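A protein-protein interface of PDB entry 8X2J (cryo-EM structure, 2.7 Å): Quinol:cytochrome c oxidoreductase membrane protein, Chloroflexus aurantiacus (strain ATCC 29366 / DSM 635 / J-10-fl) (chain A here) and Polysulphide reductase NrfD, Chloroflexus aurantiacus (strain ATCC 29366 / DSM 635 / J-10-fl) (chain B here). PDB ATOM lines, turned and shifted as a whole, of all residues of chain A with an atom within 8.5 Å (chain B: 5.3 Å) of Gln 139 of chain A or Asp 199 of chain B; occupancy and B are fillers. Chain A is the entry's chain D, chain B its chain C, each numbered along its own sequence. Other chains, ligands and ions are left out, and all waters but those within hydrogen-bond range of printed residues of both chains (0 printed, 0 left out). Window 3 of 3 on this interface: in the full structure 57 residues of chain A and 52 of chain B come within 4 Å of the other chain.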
ATOM      1  N   GLU A  11      29.985   4.474  -2.097  1.00  0.00           N
ATOM      2  CA  GLU A  11      29.187   3.293  -1.797  1.00  0.00           C
ATOM      3  C   GLU A  11      30.036   2.037  -1.936  1.00  0.00           C
ATOM      4  O   GLU A  11      30.873   1.939  -2.838  1.00  0.00           O
ATOM      5  CB  GLU A  11      27.972   3.207  -2.722  1.00  0.00           C
ATOM      6  CG  GLU A  11      26.900   2.239  -2.251  1.00  0.00           C
ATOM      7  CD  GLU A  11      25.702   2.209  -3.170  1.00  0.00           C
ATOM      8  OE1 GLU A  11      25.704   2.953  -4.171  1.00  0.00           O
ATOM      9  OE2 GLU A  11      24.762   1.435  -2.895  1.00  0.00           O
ATOM     10  N   PRO A  38      23.739  -0.618   7.853  1.00  0.00           N
ATOM     11  CA  PRO A  38      22.509  -1.074   8.524  1.00  0.00           C
ATOM     12  C   PRO A  38      22.739  -1.677   9.901  1.00  0.00           C
ATOM     13  O   PRO A  38      21.787  -1.757  10.686  1.00  0.00           O
ATOM     14  CB  PRO A  38      21.944  -2.122   7.556  1.00  0.00           C
ATOM     15  CG  PRO A  38      22.634  -1.900   6.271  1.00  0.00           C
ATOM     16  CD  PRO A  38      23.967  -1.329   6.583  1.00  0.00           C
ATOM     17  N   VAL A 132      22.935  13.866   4.499  1.00  0.00           N
ATOM     18  CA  VAL A 132      23.333  12.572   3.956  1.00  0.00           C
ATOM     19  C   VAL A 132      22.203  11.884   3.184  1.00  0.00           C
ATOM     20  O   VAL A 132      22.468  11.011   2.350  1.00  0.00           O
ATOM     21  CB  VAL A 132      23.865  11.695   5.111  1.00  0.00           C
ATOM     22  CG1 VAL A 132      22.735  11.146   5.965  1.00  0.00           C
ATOM     23  CG2 VAL A 132      24.759  10.590   4.608  1.00  0.00           C
ATOM     24  N   PHE A 133      20.948  12.282   3.401  1.00  0.00           N
ATOM     25  CA  PHE A 133      19.825  11.694   2.684  1.00  0.00           C
ATOM     26  C   PHE A 133      19.640  12.277   1.288  1.00  0.00           C
ATOM     27  O   PHE A 133      18.760  11.814   0.556  1.00  0.00           O
ATOM     28  CB  PHE A 133      18.533  11.873   3.483  1.00  0.00           C
ATOM     29  CG  PHE A 133      18.491  11.086   4.760  1.00  0.00           C
ATOM     30  CD1 PHE A 133      18.488   9.701   4.736  1.00  0.00           C
ATOM     31  CD2 PHE A 133      18.441  11.731   5.986  1.00  0.00           C
ATOM     32  CE1 PHE A 133      18.442   8.973   5.910  1.00  0.00           C
ATOM     33  CE2 PHE A 133      18.397  11.009   7.164  1.00  0.00           C
ATOM     34  CZ  PHE A 133      18.396   9.628   7.125  1.00  0.00           C
ATOM     35  N   ASN A 134      20.438  13.280   0.908  1.00  0.00           N
ATOM     36  CA  ASN A 134      20.353  13.858  -0.427  1.00  0.00           C
ATOM     37  C   ASN A 134      20.825  12.897  -1.508  1.00  0.00           C
ATOM     38  O   ASN A 134      20.441  13.057  -2.673  1.00  0.00           O
ATOM     39  CB  ASN A 134      21.171  15.148  -0.491  1.00  0.00           C
ATOM     40  CG  ASN A 134      20.423  16.338   0.065  1.00  0.00           C
ATOM     41  OD1 ASN A 134      19.314  16.646  -0.368  1.00  0.00           O
ATOM     42  ND2 ASN A 134      21.022  17.010   1.039  1.00  0.00           N
ATOM     43  N   VAL A 135      21.652  11.922  -1.158  1.00  0.00           N
ATOM     44  CA  VAL A 135      22.047  10.880  -2.111  1.00  0.00           C
ATOM     45  C   VAL A 135      20.849   9.974  -2.377  1.00  0.00           C
ATOM     46  O   VAL A 135      20.237   9.466  -1.419  1.00  0.00           O
ATOM     47  CB  VAL A 135      23.233  10.084  -1.562  1.00  0.00           C
ATOM     48  CG1 VAL A 135      23.468   8.824  -2.380  1.00  0.00           C
ATOM     49  CG2 VAL A 135      24.479  10.949  -1.552  1.00  0.00           C
ATOM     50  N   PRO A 136      20.458   9.760  -3.639  1.00  0.00           N
ATOM     51  CA  PRO A 136      19.282   8.918  -3.913  1.00  0.00           C
ATOM     52  C   PRO A 136      19.492   7.442  -3.611  1.00  0.00           C
ATOM     53  O   PRO A 136      18.501   6.712  -3.484  1.00  0.00           O
ATOM     54  CB  PRO A 136      19.026   9.148  -5.408  1.00  0.00           C
ATOM     55  CG  PRO A 136      20.355   9.535  -5.958  1.00  0.00           C
ATOM     56  CD  PRO A 136      21.049  10.308  -4.873  1.00  0.00           C
ATOM     57  N   ARG A 137      20.734   6.981  -3.490  1.00  0.00           N
ATOM     58  CA  ARG A 137      21.008   5.595  -3.141  1.00  0.00           C
ATOM     59  C   ARG A 137      21.196   5.385  -1.646  1.00  0.00           C
ATOM     60  O   ARG A 137      21.499   4.264  -1.229  1.00  0.00           O
ATOM     61  CB  ARG A 137      22.243   5.094  -3.894  1.00  0.00           C
ATOM     62  CG  ARG A 137      21.947   4.646  -5.314  1.00  0.00           C
ATOM     63  CD  ARG A 137      22.789   3.448  -5.710  1.00  0.00           C
ATOM     64  NE  ARG A 137      22.752   2.392  -4.706  1.00  0.00           N
ATOM     65  CZ  ARG A 137      21.851   1.420  -4.674  1.00  0.00           C
ATOM     66  NH1 ARG A 137      20.880   1.348  -5.568  1.00  0.00           N
ATOM     67  NH2 ARG A 137      21.928   0.497  -3.719  1.00  0.00           N
ATOM     68  N   PHE A 138      21.008   6.424  -0.831  1.00  0.00           N
ATOM     69  CA  PHE A 138      21.075   6.285   0.619  1.00  0.00           C
ATOM     70  C   PHE A 138      19.806   5.685   1.212  1.00  0.00           C
ATOM     71  O   PHE A 138      19.764   5.428   2.419  1.00  0.00           O
ATOM     72  CB  PHE A 138      21.364   7.639   1.274  1.00  0.00           C
ATOM     73  CG  PHE A 138      22.050   7.531   2.608  1.00  0.00           C
ATOM     74  CD1 PHE A 138      23.373   7.131   2.690  1.00  0.00           C
ATOM     75  CD2 PHE A 138      21.363   7.807   3.780  1.00  0.00           C
ATOM     76  CE1 PHE A 138      24.002   7.020   3.917  1.00  0.00           C
ATOM     77  CE2 PHE A 138      21.984   7.694   5.008  1.00  0.00           C
ATOM     78  CZ  PHE A 138      23.304   7.301   5.076  1.00  0.00           C
ATOM     79  N   GLN A 139      18.773   5.460   0.395  1.00  0.00           N
ATOM     80  CA  GLN A 139      17.585   4.747   0.852  1.00  0.00           C
ATOM     81  C   GLN A 139      17.903   3.302   1.219  1.00  0.00           C
ATOM     82  O   GLN A 139      17.229   2.717   2.071  1.00  0.00           O
ATOM     83  CB  GLN A 139      16.506   4.799  -0.230  1.00  0.00           C
ATOM     84  CG  GLN A 139      15.112   4.426   0.238  1.00  0.00           C
ATOM     85  CD  GLN A 139      14.274   3.827  -0.871  1.00  0.00           C
ATOM     86  OE1 GLN A 139      14.502   4.098  -2.049  1.00  0.00           O
ATOM     87  NE2 GLN A 139      13.304   2.998  -0.502  1.00  0.00           N
ATOM     88  N   TYR A 140      18.930   2.719   0.613  1.00  0.00           N
ATOM     89  CA  TYR A 140      19.315   1.343   0.883  1.00  0.00           C
ATOM     90  C   TYR A 140      20.349   1.225   1.995  1.00  0.00           C
ATOM     91  O   TYR A 140      20.833   0.121   2.251  1.00  0.00           O
ATOM     92  CB  TYR A 140      19.833   0.690  -0.397  1.00  0.00           C
ATOM     93  CG  TYR A 140      18.875   0.827  -1.556  1.00  0.00           C
ATOM     94  CD1 TYR A 140      17.747   0.023  -1.646  1.00  0.00           C
ATOM     95  CD2 TYR A 140      19.090   1.774  -2.550  1.00  0.00           C
ATOM     96  CE1 TYR A 140      16.863   0.150  -2.701  1.00  0.00           C
ATOM     97  CE2 TYR A 140      18.212   1.908  -3.610  1.00  0.00           C
ATOM     98  CZ  TYR A 140      17.102   1.094  -3.680  1.00  0.00           C
ATOM     99  OH  TYR A 140      16.229   1.228  -4.735  1.00  0.00           O
ATOM    100  N   ALA A 141      20.671   2.325   2.683  1.00  0.00           N
ATOM    101  CA  ALA A 141      21.665   2.305   3.754  1.00  0.00           C
ATOM    102  C   ALA A 141      21.207   1.545   4.992  1.00  0.00           C
ATOM    103  O   ALA A 141      22.022   1.319   5.890  1.00  0.00           O
ATOM    104  CB  ALA A 141      22.051   3.731   4.148  1.00  0.00           C
ATOM    105  N   SER A 142      19.928   1.183   5.080  1.00  0.00           N
ATOM    106  CA  SER A 142      19.446   0.187   6.025  1.00  0.00           C
ATOM    107  C   SER A 142      18.961  -1.076   5.321  1.00  0.00           C
ATOM    108  O   SER A 142      18.353  -1.940   5.959  1.00  0.00           O
ATOM    109  CB  SER A 142      18.334   0.774   6.892  1.00  0.00           C
ATOM    110  OG  SER A 142      17.278   1.267   6.090  1.00  0.00           O
ATOM    111  N   GLN A 143      19.216  -1.199   4.018  1.00  0.00           N
ATOM    112  CA  GLN A 143      18.765  -2.307   3.179  1.00  0.00           C
ATOM    113  C   GLN A 143      19.933  -2.888   2.388  1.00  0.00           C
ATOM    114  O   GLN A 143      19.878  -3.003   1.159  1.00  0.00           O
ATOM    115  CB  GLN A 143      17.664  -1.879   2.209  1.00  0.00           C
ATOM    116  CG  GLN A 143      16.536  -1.060   2.804  1.00  0.00           C
ATOM    117  CD  GLN A 143      15.555  -0.606   1.750  1.00  0.00           C
ATOM    118  OE1 GLN A 143      14.854   0.387   1.925  1.00  0.00           O
ATOM    119  NE2 GLN A 143      15.498  -1.332   0.641  1.00  0.00           N
ATOM    120  N   ASP A 144      21.020  -3.216   3.100  1.00  0.00           N
ATOM    121  CA  ASP A 144      22.264  -3.778   2.550  1.00  0.00           C
ATOM    122  C   ASP A 144      22.925  -2.825   1.548  1.00  0.00           C
ATOM    123  O   ASP A 144      23.060  -3.114   0.358  1.00  0.00           O
ATOM    124  CB  ASP A 144      22.039  -5.168   1.934  1.00  0.00           C
ATOM    125  CG  ASP A 144      23.335  -5.919   1.683  1.00  0.00           C
ATOM    126  OD1 ASP A 144      24.377  -5.530   2.250  1.00  0.00           O
ATOM    127  OD2 ASP A 144      23.312  -6.904   0.915  1.00  0.00           O
ATOM    128  N   ALA A 145      23.328  -1.666   2.061  1.00  0.00           N
ATOM    129  CA  ALA A 145      24.266  -0.797   1.370  1.00  0.00           C
ATOM    130  C   ALA A 145      25.139  -0.136   2.421  1.00  0.00           C
ATOM    131  O   ALA A 145      24.718   0.060   3.564  1.00  0.00           O
ATOM    132  CB  ALA A 145      23.575   0.258   0.501  1.00  0.00           C
ATOM    133  N   PHE A 147      28.190   2.938   3.222  1.00  0.00           N
ATOM    134  CA  PHE A 147      28.675   4.234   2.782  1.00  0.00           C
ATOM    135  C   PHE A 147      29.770   4.720   3.719  1.00  0.00           C
ATOM    136  O   PHE A 147      29.880   4.279   4.863  1.00  0.00           O
ATOM    137  CB  PHE A 147      27.544   5.269   2.722  1.00  0.00           C
ATOM    138  CG  PHE A 147      26.506   4.978   1.678  1.00  0.00           C
ATOM    139  CD1 PHE A 147      25.410   4.180   1.972  1.00  0.00           C
ATOM    140  CD2 PHE A 147      26.620   5.511   0.406  1.00  0.00           C
ATOM    141  CE1 PHE A 147      24.455   3.911   1.012  1.00  0.00           C
ATOM    142  CE2 PHE A 147      25.666   5.249  -0.558  1.00  0.00           C
ATOM    143  CZ  PHE A 147      24.584   4.448  -0.254  1.00  0.00           C
ATOM    144  N   PHE B 194      12.707   1.358  12.818  1.00  0.00           N
ATOM    145  CA  PHE B 194      11.891   2.438  12.277  1.00  0.00           C
ATOM    146  C   PHE B 194      12.558   3.063  11.061  1.00  0.00           C
ATOM    147  O   PHE B 194      11.881   3.427  10.093  1.00  0.00           O
ATOM    148  CB  PHE B 194      11.650   3.495  13.350  1.00  0.00           C
ATOM    149  CG  PHE B 194      10.533   3.170  14.290  1.00  0.00           C
ATOM    150  CD1 PHE B 194       9.318   2.720  13.811  1.00  0.00           C
ATOM    151  CD2 PHE B 194      10.697   3.326  15.657  1.00  0.00           C
ATOM    152  CE1 PHE B 194       8.287   2.431  14.678  1.00  0.00           C
ATOM    153  CE2 PHE B 194       9.669   3.039  16.528  1.00  0.00           C
ATOM    154  CZ  PHE B 194       8.465   2.585  16.039  1.00  0.00           C
ATOM    155  N   ALA B 195      13.890   3.184  11.091  1.00  0.00           N
ATOM    156  CA  ALA B 195      14.630   3.673   9.929  1.00  0.00           C
ATOM    157  C   ALA B 195      14.522   2.714   8.747  1.00  0.00           C
ATOM    158  O   ALA B 195      14.381   3.149   7.598  1.00  0.00           O
ATOM    159  CB  ALA B 195      16.093   3.901  10.300  1.00  0.00           C
ATOM    160  N   THR B 196      14.587   1.407   9.015  1.00  0.00           N
ATOM    161  CA  THR B 196      14.442   0.408   7.959  1.00  0.00           C
ATOM    162  C   THR B 196      13.045   0.434   7.346  1.00  0.00           C
ATOM    163  O   THR B 196      12.899   0.320   6.126  1.00  0.00           O
ATOM    164  CB  THR B 196      14.757  -0.985   8.502  1.00  0.00           C
ATOM    165  OG1 THR B 196      15.947  -0.933   9.298  1.00  0.00           O
ATOM    166  CG2 THR B 196      14.963  -1.968   7.362  1.00  0.00           C
ATOM    167  N   LEU B 197      12.010   0.590   8.176  1.00  0.00           N
ATOM    168  CA  LEU B 197      10.646   0.669   7.655  1.00  0.00           C
ATOM    169  C   LEU B 197      10.411   1.969   6.890  1.00  0.00           C
ATOM    170  O   LEU B 197       9.690   1.981   5.885  1.00  0.00           O
ATOM    171  CB  LEU B 197       9.640   0.539   8.794  1.00  0.00           C
ATOM    172  CG  LEU B 197       9.568  -0.804   9.513  1.00  0.00           C
ATOM    173  CD1 LEU B 197       8.632  -0.685  10.690  1.00  0.00           C
ATOM    174  CD2 LEU B 197       9.126  -1.911   8.581  1.00  0.00           C
ATOM    175  N   ARG B 198      11.008   3.071   7.360  1.00  0.00           N
ATOM    176  CA  ARG B 198      10.941   4.341   6.647  1.00  0.00           C
ATOM    177  C   ARG B 198      11.641   4.250   5.298  1.00  0.00           C
ATOM    178  O   ARG B 198      11.211   4.866   4.319  1.00  0.00           O
ATOM    179  CB  ARG B 198      11.564   5.440   7.512  1.00  0.00           C
ATOM    180  CG  ARG B 198      11.527   6.842   6.922  1.00  0.00           C
ATOM    181  CD  ARG B 198      12.924   7.347   6.592  1.00  0.00           C
ATOM    182  NE  ARG B 198      13.842   7.224   7.717  1.00  0.00           N
ATOM    183  CZ  ARG B 198      15.148   7.031   7.598  1.00  0.00           C
ATOM    184  NH1 ARG B 198      15.727   6.929   6.414  1.00  0.00           N
ATOM    185  NH2 ARG B 198      15.892   6.940   8.696  1.00  0.00           N
ATOM    186  N   ASP B 199      12.722   3.478   5.228  1.00  0.00           N
ATOM    187  CA  ASP B 199      13.408   3.285   3.958  1.00  0.00           C
ATOM    188  C   ASP B 199      12.628   2.354   3.032  1.00  0.00           C
ATOM    189  O   ASP B 199      12.594   2.569   1.815  1.00  0.00           O
ATOM    190  CB  ASP B 199      14.809   2.743   4.219  1.00  0.00           C
ATOM    191  CG  ASP B 199      15.760   3.809   4.720  1.00  0.00           C
ATOM    192  OD1 ASP B 199      15.480   5.007   4.501  1.00  0.00           O
ATOM    193  OD2 ASP B 199      16.788   3.450   5.332  1.00  0.00           O
ATOM    194  N   ARG B 200      11.994   1.320   3.587  1.00  0.00           N
ATOM    195  CA  ARG B 200      11.328   0.293   2.795  1.00  0.00           C
ATOM    196  C   ARG B 200       9.886   0.626   2.443  1.00  0.00           C
ATOM    197  O   ARG B 200       9.274  -0.121   1.672  1.00  0.00           O
ATOM    198  CB  ARG B 200      11.351  -1.046   3.537  1.00  0.00           C
ATOM    199  CG  ARG B 200      12.667  -1.789   3.460  1.00  0.00           C
ATOM    200  CD  ARG B 200      12.463  -3.285   3.623  1.00  0.00           C
ATOM    201  NE  ARG B 200      11.637  -3.839   2.559  1.00  0.00           N
ATOM    202  CZ  ARG B 200      12.113  -4.321   1.419  1.00  0.00           C
ATOM    203  NH1 ARG B 200      13.410  -4.336   1.165  1.00  0.00           N
ATOM    204  NH2 ARG B 200      11.266  -4.799   0.512  1.00  0.00           N
ATOM    205  N   ALA B 201       9.325   1.702   2.991  1.00  0.00           N
ATOM    206  CA  ALA B 201       7.944   2.058   2.701  1.00  0.00           C
ATOM    207  C   ALA B 201       7.797   2.543   1.261  1.00  0.00           C
ATOM    208  O   ALA B 201       8.768   2.909   0.594  1.00  0.00           O
ATOM    209  CB  ALA B 201       7.453   3.135   3.666  1.00  0.00           C
ATOM    210  N   LYS B 207       5.913   7.093   5.106  1.00  0.00           N
ATOM    211  CA  LYS B 207       7.311   7.416   5.382  1.00  0.00           C
ATOM    212  C   LYS B 207       7.440   8.246   6.650  1.00  0.00           C
ATOM    213  O   LYS B 207       8.329   8.004   7.474  1.00  0.00           O
ATOM    214  CB  LYS B 207       7.921   8.196   4.219  1.00  0.00           C
ATOM    215  CG  LYS B 207       7.870   7.547   2.860  1.00  0.00           C
ATOM    216  CD  LYS B 207       8.917   6.483   2.721  1.00  0.00           C
ATOM    217  CE  LYS B 207       9.115   6.101   1.275  1.00  0.00           C
ATOM    218  NZ  LYS B 207       9.800   7.180   0.518  1.00  0.00           N
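The side-chain hydroxyl (OG) of Ser 142 of chain A sits close to the side-chain carboxylate (OD2) of Asp 199 of chain B.
The backbone NH of Arg 200 of chain B is in hydrogen-bond range of the side-chain amide oxygen of Gln 143 of chain A, 3.4 Å away.
The backbone carbonyl oxygen (O) of Asp 199 of chain B lies close to the side-chain amide oxygen (OE1) of Gln 143 of chain A (3.1 Å).
NE2 of Gln 139 of chain A lies within hydrogen-bond range of O of Asp 199 of chain B (2.5 Å).
NH1 of Arg 198 of chain B is in salt-bridge range of OD1 of Asp 199 of chain B (2.7 Å).
O of Gln 139 of chain A sits close to OE1 of Gln 143 of chain A, at 3.3 Å.
Among the printed residues, pairs that only touch across the chains: Phe 133 of chain A with Arg 198 of chain B, Ser 142 of chain A with Ala 195 of chain B and Ser 142 of chain A with Thr 196 of chain B.
Of chain A, only Gln 139 (2.5 Å), Ser 142 (2.4 Å) and Gln 143 (3.1 Å) come within 4 Å of Asp 199 of chain B.
Of the printed residues of chain B, Phe 133 of chain A touches Arg 198.
Printed residues of chain A within 4 Å of Arg 200 of chain B: Gln 143 (3.4 Å).
Of the printed residues of chain B, Gln 143 of chain A touches Asp 199 (3.1 Å) and Arg 200 (3.4 Å).
The nearest residue of chain B that does not touch Gln 139 of chain A is Arg 200 of chain B (4.6 Å).
Hydrophobic or aromatic side chains of chain A that line the printed part of chain B: Phe 133.
Printed residues of chain B that touch a printed residue of chain A: Ala 195, Thr 196, Arg 198, Asp 199 and Arg 200.
Among the printed residues, no Asp or Glu carboxylate lies within 4 Å of a Lys or Arg side-chain nitrogen of the other chain.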
